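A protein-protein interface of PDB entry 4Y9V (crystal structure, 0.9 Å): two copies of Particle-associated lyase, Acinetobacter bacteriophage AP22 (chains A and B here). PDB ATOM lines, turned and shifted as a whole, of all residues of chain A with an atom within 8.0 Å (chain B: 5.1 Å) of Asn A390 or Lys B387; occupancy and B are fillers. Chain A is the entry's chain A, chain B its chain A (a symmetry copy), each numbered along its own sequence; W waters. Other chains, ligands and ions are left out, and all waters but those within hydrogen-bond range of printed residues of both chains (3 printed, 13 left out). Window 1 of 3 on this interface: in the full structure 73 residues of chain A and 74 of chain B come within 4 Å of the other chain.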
ATOM      1  N   ASP A 346     -39.362   3.024   4.915  1.00  0.00           N
ATOM      2  CA  ASP A 346     -38.363   3.731   4.096  1.00  0.00           C
ATOM      3  C   ASP A 346     -38.396   5.195   4.434  1.00  0.00           C
ATOM      4  O   ASP A 346     -39.458   5.821   4.485  1.00  0.00           O
ATOM      5  CB  ASP A 346     -38.685   3.522   2.617  1.00  0.00           C
ATOM      6  CG  ASP A 346     -37.624   4.065   1.673  1.00  0.00           C
ATOM      7  OD1 ASP A 346     -36.436   3.963   1.949  1.00  0.00           O
ATOM      8  OD2 ASP A 346     -37.986   4.496   0.563  1.00  0.00           O
ATOM      9  N   HIS A 347     -37.220   5.800   4.702  1.00  0.00           N
ATOM     10  CA  HIS A 347     -37.176   7.248   4.995  1.00  0.00           C
ATOM     11  C   HIS A 347     -38.057   7.582   6.186  1.00  0.00           C
ATOM     12  O   HIS A 347     -38.707   8.634   6.227  1.00  0.00           O
ATOM     13  CB  HIS A 347     -37.481   8.094   3.741  1.00  0.00           C
ATOM     14  CG  HIS A 347     -36.287   8.190   2.807  1.00  0.00           C
ATOM     15  ND1 HIS A 347     -36.024   7.559   1.645  1.00  0.00           N
ATOM     16  CD2 HIS A 347     -35.198   8.960   3.057  1.00  0.00           C
ATOM     17  CE1 HIS A 347     -34.810   7.986   1.182  1.00  0.00           C
ATOM     18  NE2 HIS A 347     -34.314   8.809   2.044  1.00  0.00           N
ATOM     19  N   GLU A 361     -37.795  -4.956   5.382  1.00  0.00           N
ATOM     20  CA  GLU A 361     -36.717  -3.973   5.223  1.00  0.00           C
ATOM     21  C   GLU A 361     -36.980  -2.719   6.033  1.00  0.00           C
ATOM     22  O   GLU A 361     -38.111  -2.231   6.102  1.00  0.00           O
ATOM     23  CB  GLU A 361     -36.577  -3.609   3.730  1.00  0.00           C
ATOM     24  CG  GLU A 361     -35.471  -2.613   3.397  1.00  0.00           C
ATOM     25  CD  GLU A 361     -35.165  -2.510   1.906  1.00  0.00           C
ATOM     26  OE1 GLU A 361     -36.091  -2.753   1.098  1.00  0.00           O
ATOM     27  OE2 GLU A 361     -34.023  -2.154   1.565  1.00  0.00           O
ATOM     28  N   TYR A 362     -35.906  -2.187   6.611  1.00  0.00           N
ATOM     29  CA  TYR A 362     -35.818  -0.774   7.001  1.00  0.00           C
ATOM     30  C   TYR A 362     -34.750  -0.154   6.101  1.00  0.00           C
ATOM     31  O   TYR A 362     -33.610  -0.657   6.087  1.00  0.00           O
ATOM     32  CB  TYR A 362     -35.431  -0.541   8.469  1.00  0.00           C
ATOM     33  CG  TYR A 362     -36.512  -0.927   9.461  1.00  0.00           C
ATOM     34  CD1 TYR A 362     -36.710  -2.243   9.851  1.00  0.00           C
ATOM     35  CD2 TYR A 362     -37.347   0.038   9.989  1.00  0.00           C
ATOM     36  CE1 TYR A 362     -37.702  -2.580  10.750  1.00  0.00           C
ATOM     37  CE2 TYR A 362     -38.345  -0.288  10.900  1.00  0.00           C
ATOM     38  CZ  TYR A 362     -38.540  -1.617  11.270  1.00  0.00           C
ATOM     39  OH  TYR A 362     -39.537  -1.875  12.157  1.00  0.00           O
ATOM     40  N   SER A 363     -35.101   0.882   5.357  1.00  0.00           N
ATOM     41  CA  SER A 363     -34.157   1.536   4.449  1.00  0.00           C
ATOM     42  C   SER A 363     -34.207   3.040   4.654  1.00  0.00           C
ATOM     43  O   SER A 363     -35.272   3.619   4.845  1.00  0.00           O
ATOM     44  CB  SER A 363     -34.458   1.187   2.993  1.00  0.00           C
ATOM     45  OG  SER A 363     -35.807   1.455   2.647  1.00  0.00           O
ATOM     46  N   ASN A 364     -33.030   3.666   4.587  1.00  0.00           N
ATOM     47  CA  ASN A 364     -32.955   5.125   4.645  1.00  0.00           C
ATOM     48  C   ASN A 364     -33.628   5.684   5.912  1.00  0.00           C
ATOM     49  O   ASN A 364     -34.125   6.823   5.863  1.00  0.00           O
ATOM     50  CB  ASN A 364     -33.555   5.765   3.387  1.00  0.00           C
ATOM     51  CG  ASN A 364     -32.859   5.242   2.149  1.00  0.00           C
ATOM     52  OD1 ASN A 364     -31.658   5.374   2.012  1.00  0.00           O
ATOM     53  ND2 ASN A 364     -33.659   4.610   1.283  1.00  0.00           N
ATOM     54  N   CYS A 365     -33.617   4.932   6.978  1.00  0.00           N
ATOM     55  CA  CYS A 365     -34.275   5.338   8.215  1.00  0.00           C
ATOM     56  C   CYS A 365     -33.268   5.880   9.234  1.00  0.00           C
ATOM     57  O   CYS A 365     -32.115   5.460   9.248  1.00  0.00           O
ATOM     58  CB  CYS A 365     -34.999   4.159   8.886  1.00  0.00           C
ATOM     59  SG  CYS A 365     -36.489   3.584   8.001  1.00  0.00           S
ATOM     60  N   ASP A 366     -33.772   6.738  10.107  1.00  0.00           N
ATOM     61  CA  ASP A 366     -33.081   7.184  11.306  1.00  0.00           C
ATOM     62  C   ASP A 366     -33.605   6.318  12.448  1.00  0.00           C
ATOM     63  O   ASP A 366     -34.800   6.394  12.755  1.00  0.00           O
ATOM     64  CB  ASP A 366     -33.374   8.658  11.615  1.00  0.00           C
ATOM     65  CG  ASP A 366     -32.634   9.643  10.748  1.00  0.00           C
ATOM     66  OD1 ASP A 366     -32.911  10.840  10.896  1.00  0.00           O
ATOM     67  OD2 ASP A 366     -31.757   9.183   9.991  1.00  0.00           O
ATOM     68  N   ILE A 367     -32.731   5.497  13.028  1.00  0.00           N
ATOM     69  CA  ILE A 367     -33.141   4.528  14.036  1.00  0.00           C
ATOM     70  C   ILE A 367     -32.354   4.797  15.313  1.00  0.00           C
ATOM     71  O   ILE A 367     -31.137   4.649  15.358  1.00  0.00           O
ATOM     72  CB  ILE A 367     -32.941   3.070  13.581  1.00  0.00           C
ATOM     73  CG1 ILE A 367     -33.610   2.814  12.215  1.00  0.00           C
ATOM     74  CG2 ILE A 367     -33.473   2.129  14.659  1.00  0.00           C
ATOM     75  CD1 ILE A 367     -33.355   1.461  11.643  1.00  0.00           C
ATOM     76  N   LYS A 387     -33.494  -6.906   5.604  1.00  0.00           N
ATOM     77  CA  LYS A 387     -32.667  -5.946   4.873  1.00  0.00           C
ATOM     78  C   LYS A 387     -32.606  -4.618   5.622  1.00  0.00           C
ATOM     79  O   LYS A 387     -33.642  -4.036   5.966  1.00  0.00           O
ATOM     80  CB  LYS A 387     -33.241  -5.693   3.478  1.00  0.00           C
ATOM     81  CG  LYS A 387     -33.253  -6.889   2.562  1.00  0.00           C
ATOM     82  CD  LYS A 387     -33.961  -6.692   1.239  1.00  0.00           C
ATOM     83  CE  LYS A 387     -33.236  -5.815   0.330  1.00  0.00           C
ATOM     84  NZ  LYS A 387     -33.556  -5.742  -1.122  1.00  0.00           N
ATOM     85  N   LEU A 388     -31.393  -4.140   5.853  1.00  0.00           N
ATOM     86  CA  LEU A 388     -31.140  -2.876   6.533  1.00  0.00           C
ATOM     87  C   LEU A 388     -30.276  -2.030   5.592  1.00  0.00           C
ATOM     88  O   LEU A 388     -29.061  -2.181   5.561  1.00  0.00           O
ATOM     89  CB  LEU A 388     -30.448  -3.122   7.853  1.00  0.00           C
ATOM     90  CG  LEU A 388     -31.306  -3.805   8.920  1.00  0.00           C
ATOM     91  CD1 LEU A 388     -30.471  -4.208  10.099  1.00  0.00           C
ATOM     92  CD2 LEU A 388     -32.459  -2.888   9.358  1.00  0.00           C
ATOM     93  N   THR A 389     -30.929  -1.165   4.811  1.00  0.00           N
ATOM     94  CA  THR A 389     -30.302  -0.563   3.659  1.00  0.00           C
ATOM     95  C   THR A 389     -30.111   0.930   3.903  1.00  0.00           C
ATOM     96  O   THR A 389     -31.085   1.696   3.946  1.00  0.00           O
ATOM     97  CB  THR A 389     -31.130  -0.813   2.406  1.00  0.00           C
ATOM     98  OG1 THR A 389     -31.462  -2.193   2.370  1.00  0.00           O
ATOM     99  CG2 THR A 389     -30.363  -0.409   1.157  1.00  0.00           C
ATOM    100  N   ASN A 390     -28.863   1.371   4.066  1.00  0.00           N
ATOM    101  CA  ASN A 390     -28.574   2.801   4.124  1.00  0.00           C
ATOM    102  C   ASN A 390     -29.271   3.513   5.274  1.00  0.00           C
ATOM    103  O   ASN A 390     -29.658   4.687   5.132  1.00  0.00           O
ATOM    104  CB  ASN A 390     -28.803   3.472   2.791  1.00  0.00           C
ATOM    105  CG  ASN A 390     -27.712   4.453   2.488  1.00  0.00           C
ATOM    106  OD1 ASN A 390     -26.924   4.832   3.345  1.00  0.00           O
ATOM    107  ND2 ASN A 390     -27.687   4.903   1.261  1.00  0.00           N
ATOM    108  N   ASN A 391     -29.395   2.862   6.435  1.00  0.00           N
ATOM    109  CA  ASN A 391     -29.944   3.536   7.608  1.00  0.00           C
ATOM    110  C   ASN A 391     -28.847   4.310   8.349  1.00  0.00           C
ATOM    111  O   ASN A 391     -27.662   4.015   8.216  1.00  0.00           O
ATOM    112  CB  ASN A 391     -30.580   2.523   8.564  1.00  0.00           C
ATOM    113  CG  ASN A 391     -31.697   1.749   7.909  1.00  0.00           C
ATOM    114  OD1 ASN A 391     -32.616   2.308   7.295  1.00  0.00           O
ATOM    115  ND2 ASN A 391     -31.633   0.418   8.033  1.00  0.00           N
ATOM    116  N   THR A 392     -29.309   5.245   9.182  1.00  0.00           N
ATOM    117  CA  THR A 392     -28.461   5.941  10.145  1.00  0.00           C
ATOM    118  C   THR A 392     -28.912   5.488  11.540  1.00  0.00           C
ATOM    119  O   THR A 392     -30.091   5.581  11.861  1.00  0.00           O
ATOM    120  CB  THR A 392     -28.563   7.448   9.987  1.00  0.00           C
ATOM    121  OG1 THR A 392     -28.153   7.777   8.657  1.00  0.00           O
ATOM    122  CG2 THR A 392     -27.661   8.147  10.968  1.00  0.00           C
ATOM    123  N   TYR A 393     -27.962   5.004  12.316  1.00  0.00           N
ATOM    124  CA  TYR A 393     -28.235   4.449  13.640  1.00  0.00           C
ATOM    125  C   TYR A 393     -27.611   5.361  14.676  1.00  0.00           C
ATOM    126  O   TYR A 393     -26.443   5.750  14.542  1.00  0.00           O
ATOM    127  CB  TYR A 393     -27.629   3.038  13.782  1.00  0.00           C
ATOM    128  CG  TYR A 393     -27.999   2.088  12.662  1.00  0.00           C
ATOM    129  CD1 TYR A 393     -27.284   2.087  11.473  1.00  0.00           C
ATOM    130  CD2 TYR A 393     -29.057   1.175  12.790  1.00  0.00           C
ATOM    131  CE1 TYR A 393     -27.587   1.221  10.430  1.00  0.00           C
ATOM    132  CE2 TYR A 393     -29.378   0.315  11.755  1.00  0.00           C
ATOM    133  CZ  TYR A 393     -28.642   0.338  10.576  1.00  0.00           C
ATOM    134  OH  TYR A 393     -29.026  -0.500   9.541  1.00  0.00           O
ATOM    135  N   LYS A 420     -29.091  -8.714   5.918  1.00  0.00           N
ATOM    136  CA  LYS A 420     -28.369  -8.019   4.846  1.00  0.00           C
ATOM    137  C   LYS A 420     -28.291  -6.529   5.187  1.00  0.00           C
ATOM    138  O   LYS A 420     -29.244  -5.797   4.971  1.00  0.00           O
ATOM    139  CB  LYS A 420     -29.020  -8.228   3.479  1.00  0.00           C
ATOM    140  CG  LYS A 420     -28.144  -7.908   2.288  1.00  0.00           C
ATOM    141  CD  LYS A 420     -28.687  -8.418   0.933  1.00  0.00           C
ATOM    142  CE  LYS A 420     -27.689  -8.249  -0.171  1.00  0.00           C
ATOM    143  NZ  LYS A 420     -28.260  -8.797  -1.436  1.00  0.00           N
ATOM    144  N   LEU A 421     -27.142  -6.101   5.755  1.00  0.00           N
ATOM    145  CA  LEU A 421     -26.917  -4.718   6.185  1.00  0.00           C
ATOM    146  C   LEU A 421     -26.000  -4.113   5.125  1.00  0.00           C
ATOM    147  O   LEU A 421     -24.846  -4.491   5.017  1.00  0.00           O
ATOM    148  CB  LEU A 421     -26.328  -4.711   7.592  1.00  0.00           C
ATOM    149  CG  LEU A 421     -26.335  -3.355   8.308  1.00  0.00           C
ATOM    150  CD1 LEU A 421     -25.925  -3.586   9.774  1.00  0.00           C
ATOM    151  CD2 LEU A 421     -25.432  -2.305   7.680  1.00  0.00           C
ATOM    152  N   ASP A 422     -26.583  -3.226   4.324  1.00  0.00           N
ATOM    153  CA  ASP A 422     -25.965  -2.689   3.113  1.00  0.00           C
ATOM    154  C   ASP A 422     -25.900  -1.175   3.233  1.00  0.00           C
ATOM    155  O   ASP A 422     -26.912  -0.491   3.073  1.00  0.00           O
ATOM    156  CB  ASP A 422     -26.775  -3.119   1.910  1.00  0.00           C
ATOM    157  CG  ASP A 422     -26.308  -2.677   0.582  1.00  0.00           C
ATOM    158  OD1 ASP A 422     -25.184  -2.178   0.462  1.00  0.00           O
ATOM    159  OD2 ASP A 422     -27.128  -2.822  -0.405  1.00  0.00           O
ATOM    160  N   GLY A 423     -24.717  -0.658   3.537  1.00  0.00           N
ATOM    161  CA  GLY A 423     -24.510   0.748   3.670  1.00  0.00           C
ATOM    162  C   GLY A 423     -25.077   1.324   4.970  1.00  0.00           C
ATOM    163  O   GLY A 423     -25.656   0.651   5.784  1.00  0.00           O
ATOM    164  N   GLY A 424     -24.885   2.633   5.107  1.00  0.00           N
ATOM    165  CA  GLY A 424     -25.400   3.414   6.195  1.00  0.00           C
ATOM    166  C   GLY A 424     -24.295   3.922   7.114  1.00  0.00           C
ATOM    167  O   GLY A 424     -23.099   3.867   6.800  1.00  0.00           O
ATOM    168  N   CYS A 425     -24.739   4.464   8.255  1.00  0.00           N
ATOM    169  CA  CYS A 425     -23.890   5.192   9.181  1.00  0.00           C
ATOM    170  C   CYS A 425     -24.268   4.792  10.613  1.00  0.00           C
ATOM    171  O   CYS A 425     -25.392   5.044  11.040  1.00  0.00           O
ATOM    172  CB  CYS A 425     -24.087   6.683   8.963  1.00  0.00           C
ATOM    173  SG  CYS A 425     -23.089   7.677  10.077  1.00  0.00           S
ATOM    174  N   THR A 458     -22.102  -5.030   4.041  1.00  0.00           N
ATOM    175  CA  THR A 458     -21.434  -4.550   2.850  1.00  0.00           C
ATOM    176  C   THR A 458     -21.803  -3.088   2.601  1.00  0.00           C
ATOM    177  O   THR A 458     -22.448  -2.439   3.434  1.00  0.00           O
ATOM    178  CB  THR A 458     -21.810  -5.488   1.671  1.00  0.00           C
ATOM    179  OG1 THR A 458     -20.934  -5.234   0.574  1.00  0.00           O
ATOM    180  CG2 THR A 458     -23.255  -5.368   1.239  1.00  0.00           C
ATOM    181  N   GLY A 459     -21.418  -2.573   1.431  1.00  0.00           N
ATOM    182  CA  GLY A 459     -21.923  -1.284   1.011  1.00  0.00           C
ATOM    183  C   GLY A 459     -21.275  -0.085   1.622  1.00  0.00           C
ATOM    184  O   GLY A 459     -21.818   1.016   1.561  1.00  0.00           O
ATOM    185  N   GLY A 460     -20.102  -0.272   2.269  1.00  0.00           N
ATOM    186  CA  GLY A 460     -19.396   0.878   2.804  1.00  0.00           C
ATOM    187  C   GLY A 460     -20.041   1.466   4.034  1.00  0.00           C
ATOM    188  O   GLY A 460     -19.867   2.655   4.313  1.00  0.00           O
ATOM    189  N   VAL A 461     -20.759   0.652   4.790  1.00  0.00           N
ATOM    190  CA  VAL A 461     -21.309   1.081   6.061  1.00  0.00           C
ATOM    191  C   VAL A 461     -20.177   1.545   6.970  1.00  0.00           C
ATOM    192  O   VAL A 461     -19.145   0.863   7.100  1.00  0.00           O
ATOM    193  CB  VAL A 461     -22.148  -0.031   6.704  1.00  0.00           C
ATOM    194  CG1 VAL A 461     -21.393  -1.352   6.891  1.00  0.00           C
ATOM    195  CG2 VAL A 461     -22.742   0.444   8.042  1.00  0.00           C
ATOM    196  N   PHE B 355     -27.235  22.352  -0.737  1.00  0.00           N
ATOM    197  CA  PHE B 355     -27.180  21.148   0.127  1.00  0.00           C
ATOM    198  C   PHE B 355     -27.399  21.377   1.610  1.00  0.00           C
ATOM    199  O   PHE B 355     -27.314  20.428   2.382  1.00  0.00           O
ATOM    200  CB  PHE B 355     -25.866  20.388  -0.105  1.00  0.00           C
ATOM    201  CG  PHE B 355     -25.978  18.905  -0.279  1.00  0.00           C
ATOM    202  CD1 PHE B 355     -24.941  18.228  -0.924  1.00  0.00           C
ATOM    203  CD2 PHE B 355     -27.045  18.146   0.209  1.00  0.00           C
ATOM    204  CE1 PHE B 355     -24.972  16.845  -1.074  1.00  0.00           C
ATOM    205  CE2 PHE B 355     -27.081  16.786   0.044  1.00  0.00           C
ATOM    206  CZ  PHE B 355     -26.048  16.118  -0.585  1.00  0.00           C
ATOM    207  N   ASN B 360     -28.089  15.642   4.995  1.00  0.00           N
ATOM    208  CA  ASN B 360     -29.033  15.828   3.906  1.00  0.00           C
ATOM    209  C   ASN B 360     -28.669  14.901   2.753  1.00  0.00           C
ATOM    210  O   ASN B 360     -27.544  14.406   2.677  1.00  0.00           O
ATOM    211  CB  ASN B 360     -29.044  17.281   3.433  1.00  0.00           C
ATOM    212  CG  ASN B 360     -29.596  18.234   4.478  1.00  0.00           C
ATOM    213  OD1 ASN B 360     -30.535  17.898   5.212  1.00  0.00           O
ATOM    214  ND2 ASN B 360     -29.017  19.428   4.558  1.00  0.00           N
ATOM    215  N   GLU B 361     -29.621  14.718   1.834  1.00  0.00           N
ATOM    216  CA  GLU B 361     -29.414  13.789   0.716  1.00  0.00           C
ATOM    217  C   GLU B 361     -30.136  14.250  -0.535  1.00  0.00           C
ATOM    218  O   GLU B 361     -31.270  14.733  -0.474  1.00  0.00           O
ATOM    219  CB  GLU B 361     -29.916  12.387   1.121  1.00  0.00           C
ATOM    220  CG  GLU B 361     -29.740  11.298   0.068  1.00  0.00           C
ATOM    221  CD  GLU B 361     -29.961   9.885   0.601  1.00  0.00           C
ATOM    222  OE1 GLU B 361     -30.741   9.738   1.570  1.00  0.00           O
ATOM    223  OE2 GLU B 361     -29.385   8.945   0.027  1.00  0.00           O
ATOM    224  N   TYR B 362     -29.472  14.056  -1.671  1.00  0.00           N
ATOM    225  CA  TYR B 362     -30.129  13.953  -2.980  1.00  0.00           C
ATOM    226  C   TYR B 362     -29.913  12.515  -3.448  1.00  0.00           C
ATOM    227  O   TYR B 362     -28.749  12.077  -3.529  1.00  0.00           O
ATOM    228  CB  TYR B 362     -29.581  14.914  -4.045  1.00  0.00           C
ATOM    229  CG  TYR B 362     -29.921  16.372  -3.795  1.00  0.00           C
ATOM    230  CD1 TYR B 362     -29.198  17.147  -2.901  1.00  0.00           C
ATOM    231  CD2 TYR B 362     -30.986  16.958  -4.450  1.00  0.00           C
ATOM    232  CE1 TYR B 362     -29.523  18.471  -2.680  1.00  0.00           C
ATOM    233  CE2 TYR B 362     -31.318  18.291  -4.239  1.00  0.00           C
ATOM    234  CZ  TYR B 362     -30.591  19.053  -3.327  1.00  0.00           C
ATOM    235  OH  TYR B 362     -30.968  20.348  -3.157  1.00  0.00           O
ATOM    236  N   GLU B 385     -23.398  14.535   7.314  1.00  0.00           N
ATOM    237  CA  GLU B 385     -23.242  13.859   6.038  1.00  0.00           C
ATOM    238  C   GLU B 385     -23.994  14.586   4.927  1.00  0.00           C
ATOM    239  O   GLU B 385     -25.105  15.078   5.103  1.00  0.00           O
ATOM    240  CB  GLU B 385     -23.776  12.420   6.073  1.00  0.00           C
ATOM    241  CG  GLU B 385     -22.980  11.504   6.953  1.00  0.00           C
ATOM    242  CD  GLU B 385     -23.253  10.016   6.886  1.00  0.00           C
ATOM    243  OE1 GLU B 385     -24.370   9.627   6.563  1.00  0.00           O
ATOM    244  OE2 GLU B 385     -22.276   9.251   7.103  1.00  0.00           O
ATOM    245  N   PHE B 386     -23.368  14.601   3.773  1.00  0.00           N
ATOM    246  CA  PHE B 386     -23.949  15.128   2.538  1.00  0.00           C
ATOM    247  C   PHE B 386     -23.977  13.943   1.556  1.00  0.00           C
ATOM    248  O   PHE B 386     -22.932  13.591   0.998  1.00  0.00           O
ATOM    249  CB  PHE B 386     -23.153  16.287   2.024  1.00  0.00           C
ATOM    250  CG  PHE B 386     -23.202  17.485   2.936  1.00  0.00           C
ATOM    251  CD1 PHE B 386     -22.286  17.647   3.989  1.00  0.00           C
ATOM    252  CD2 PHE B 386     -24.152  18.477   2.759  1.00  0.00           C
ATOM    253  CE1 PHE B 386     -22.351  18.758   4.783  1.00  0.00           C
ATOM    254  CE2 PHE B 386     -24.217  19.598   3.561  1.00  0.00           C
ATOM    255  CZ  PHE B 386     -23.308  19.752   4.573  1.00  0.00           C
ATOM    256  N   LYS B 387     -25.126  13.310   1.435  1.00  0.00           N
ATOM    257  CA  LYS B 387     -25.249  12.039   0.724  1.00  0.00           C
ATOM    258  C   LYS B 387     -25.782  12.269  -0.688  1.00  0.00           C
ATOM    259  O   LYS B 387     -26.826  12.906  -0.874  1.00  0.00           O
ATOM    260  CB  LYS B 387     -26.206  11.099   1.459  1.00  0.00           C
ATOM    261  CG  LYS B 387     -25.756  10.669   2.831  1.00  0.00           C
ATOM    262  CD  LYS B 387     -26.764   9.871   3.629  1.00  0.00           C
ATOM    263  CE  LYS B 387     -26.963   8.524   3.110  1.00  0.00           C
ATOM    264  NZ  LYS B 387     -27.636   7.461   3.907  1.00  0.00           N
ATOM    265  N   LEU B 388     -25.072  11.734  -1.669  1.00  0.00           N
ATOM    266  CA  LEU B 388     -25.439  11.829  -3.076  1.00  0.00           C
ATOM    267  C   LEU B 388     -25.523  10.397  -3.612  1.00  0.00           C
ATOM    268  O   LEU B 388     -24.512   9.813  -3.984  1.00  0.00           O
ATOM    269  CB  LEU B 388     -24.416  12.647  -3.828  1.00  0.00           C
ATOM    270  CG  LEU B 388     -24.391  14.137  -3.480  1.00  0.00           C
ATOM    271  CD1 LEU B 388     -23.202  14.811  -4.102  1.00  0.00           C
ATOM    272  CD2 LEU B 388     -25.695  14.819  -3.921  1.00  0.00           C
ATOM    273  N   THR B 389     -26.736   9.838  -3.615  1.00  0.00           N
ATOM    274  CA  THR B 389     -26.913   8.414  -3.765  1.00  0.00           C
ATOM    275  C   THR B 389     -27.577   8.119  -5.105  1.00  0.00           C
ATOM    276  O   THR B 389     -28.761   8.427  -5.308  1.00  0.00           O
ATOM    277  CB  THR B 389     -27.732   7.853  -2.610  1.00  0.00           C
ATOM    278  OG1 THR B 389     -27.188   8.360  -1.402  1.00  0.00           O
ATOM    279  CG2 THR B 389     -27.713   6.333  -2.617  1.00  0.00           C
ATOM    280  N   LYS B 420     -20.612  11.889   0.842  1.00  0.00           N
ATOM    281  CA  LYS B 420     -20.749  10.459   0.543  1.00  0.00           C
ATOM    282  C   LYS B 420     -21.473  10.300  -0.795  1.00  0.00           C
ATOM    283  O   LYS B 420     -22.689  10.393  -0.854  1.00  0.00           O
ATOM    284  CB  LYS B 420     -21.487   9.705   1.651  1.00  0.00           C
ATOM    285  CG  LYS B 420     -21.319   8.202   1.633  1.00  0.00           C
ATOM    286  CD  LYS B 420     -21.794   7.486   2.920  1.00  0.00           C
ATOM    287  CE  LYS B 420     -21.421   6.035   2.925  1.00  0.00           C
ATOM    288  NZ  LYS B 420     -21.872   5.419   4.207  1.00  0.00           N
ATOM    289  N   ASP B 422     -22.329   7.852  -3.597  1.00  0.00           N
ATOM    290  CA  ASP B 422     -22.491   6.401  -3.662  1.00  0.00           C
ATOM    291  C   ASP B 422     -23.296   6.059  -4.905  1.00  0.00           C
ATOM    292  O   ASP B 422     -24.515   6.240  -4.931  1.00  0.00           O
ATOM    293  CB  ASP B 422     -23.177   5.921  -2.403  1.00  0.00           C
ATOM    294  CG  ASP B 422     -23.430   4.473  -2.276  1.00  0.00           C
ATOM    295  OD1 ASP B 422     -22.893   3.685  -3.061  1.00  0.00           O
ATOM    296  OD2 ASP B 422     -24.234   4.099  -1.336  1.00  0.00           O
HETATM  297  O   HOH W   1     -30.398   7.605   3.249  1.00  0.00           O
HETATM  298  O   HOH W   2     -29.741   7.107   6.448  1.00  0.00           O
HETATM  299  O   HOH W   3     -30.585   6.526  -0.306  1.00  0.00           O
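Water W3 lies within hydrogen-bond range of OE2 of Glu B361 (2.7 Å) and OD1 of Asn A364 (2.8 Å).
Water W1 lies within hydrogen-bond range of the side-chain carboxylate of Glu B361, the side-chain amino group of Lys B387 and the side-chain amide oxygen of Asn A364.
Water W2 lies within hydrogen-bond range of the backbone carbonyl oxygen of Asn A390 (2.8 Å), the side-chain hydroxyl of Thr A392 (2.8 Å) and the side-chain amino group of Lys B387 (3.3 Å).
Of the 11 printed residues of chain B, 4 touch a printed residue of chain A.
Along chain B the printed residues that touch a printed residue of chain A span positions 361 to 420.
Printed residues of chain A that touch a printed residue of chain B: His A347, Asn A390, Gly A424, Cys A425 and Gly A460.
The backbone NH (N) of Asn B360 lies within hydrogen-bond range of the backbone carbonyl oxygen (O) of Glu B385, 3.0 Å away.
The backbone NH (N) of His A347 is in hydrogen-bond range of the backbone carbonyl oxygen (O) of Ser A363 (2.9 Å).
N of Tyr B362 lies within hydrogen-bond range of O of Lys B387 (3.0 Å).
O of Asn B360 sits at hydrogen-bond distance from N of Lys B387 (2.9 Å).
The backbone NH (N) of Cys A425 sits at hydrogen-bond distance from the backbone carbonyl oxygen (O) of Asn A391 (3.0 Å).
The side-chain hydroxyl (OG1) of Thr B389 sits at hydrogen-bond distance from the side-chain carboxylate (OE2) of Glu B361.
Positions printed for both chains: 361, 362, 387, 388, 389, 420 and 422.
Of the 5 pairs that touch across the chains among the printed residues, none has its exchanged pair printed and touching as well.
O of Gly A460 lies within hydrogen-bond range of NZ of Lys B420 (3.4 Å).
The side-chain sulfur (SG) of Cys A425 is in hydrogen-bond range of the side-chain carboxylate (OE2) of Glu B385.
OD1 of Asn A390 sits at hydrogen-bond distance from NZ of Lys B387, at 2.8 Å.
The side-chain amino group of Lys B420 is in hydrogen-bond range of the backbone carbonyl oxygen of Gly A424.
Among the printed residues, pairs that only touch across the chains: His A347 with Glu B361 (3.7 Å).
Of the printed residues of chain B, His A347 touches Glu B361 (3.7 Å).
Lys A420 touches none of the printed residues of chain B.
Of the printed residues of chain B, Cys A425 touches Glu B385.
Printed residues of chain B within 4 Å of Gly A460: Lys B420 (3.4 Å).
Of the printed residues of chain A, Lys B420 touches Gly A424 (3.3 Å) and Gly A460 (3.4 Å).
The nearest printed residue of chain B that does not touch Asn A390 is Thr B389 (4.1 Å).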
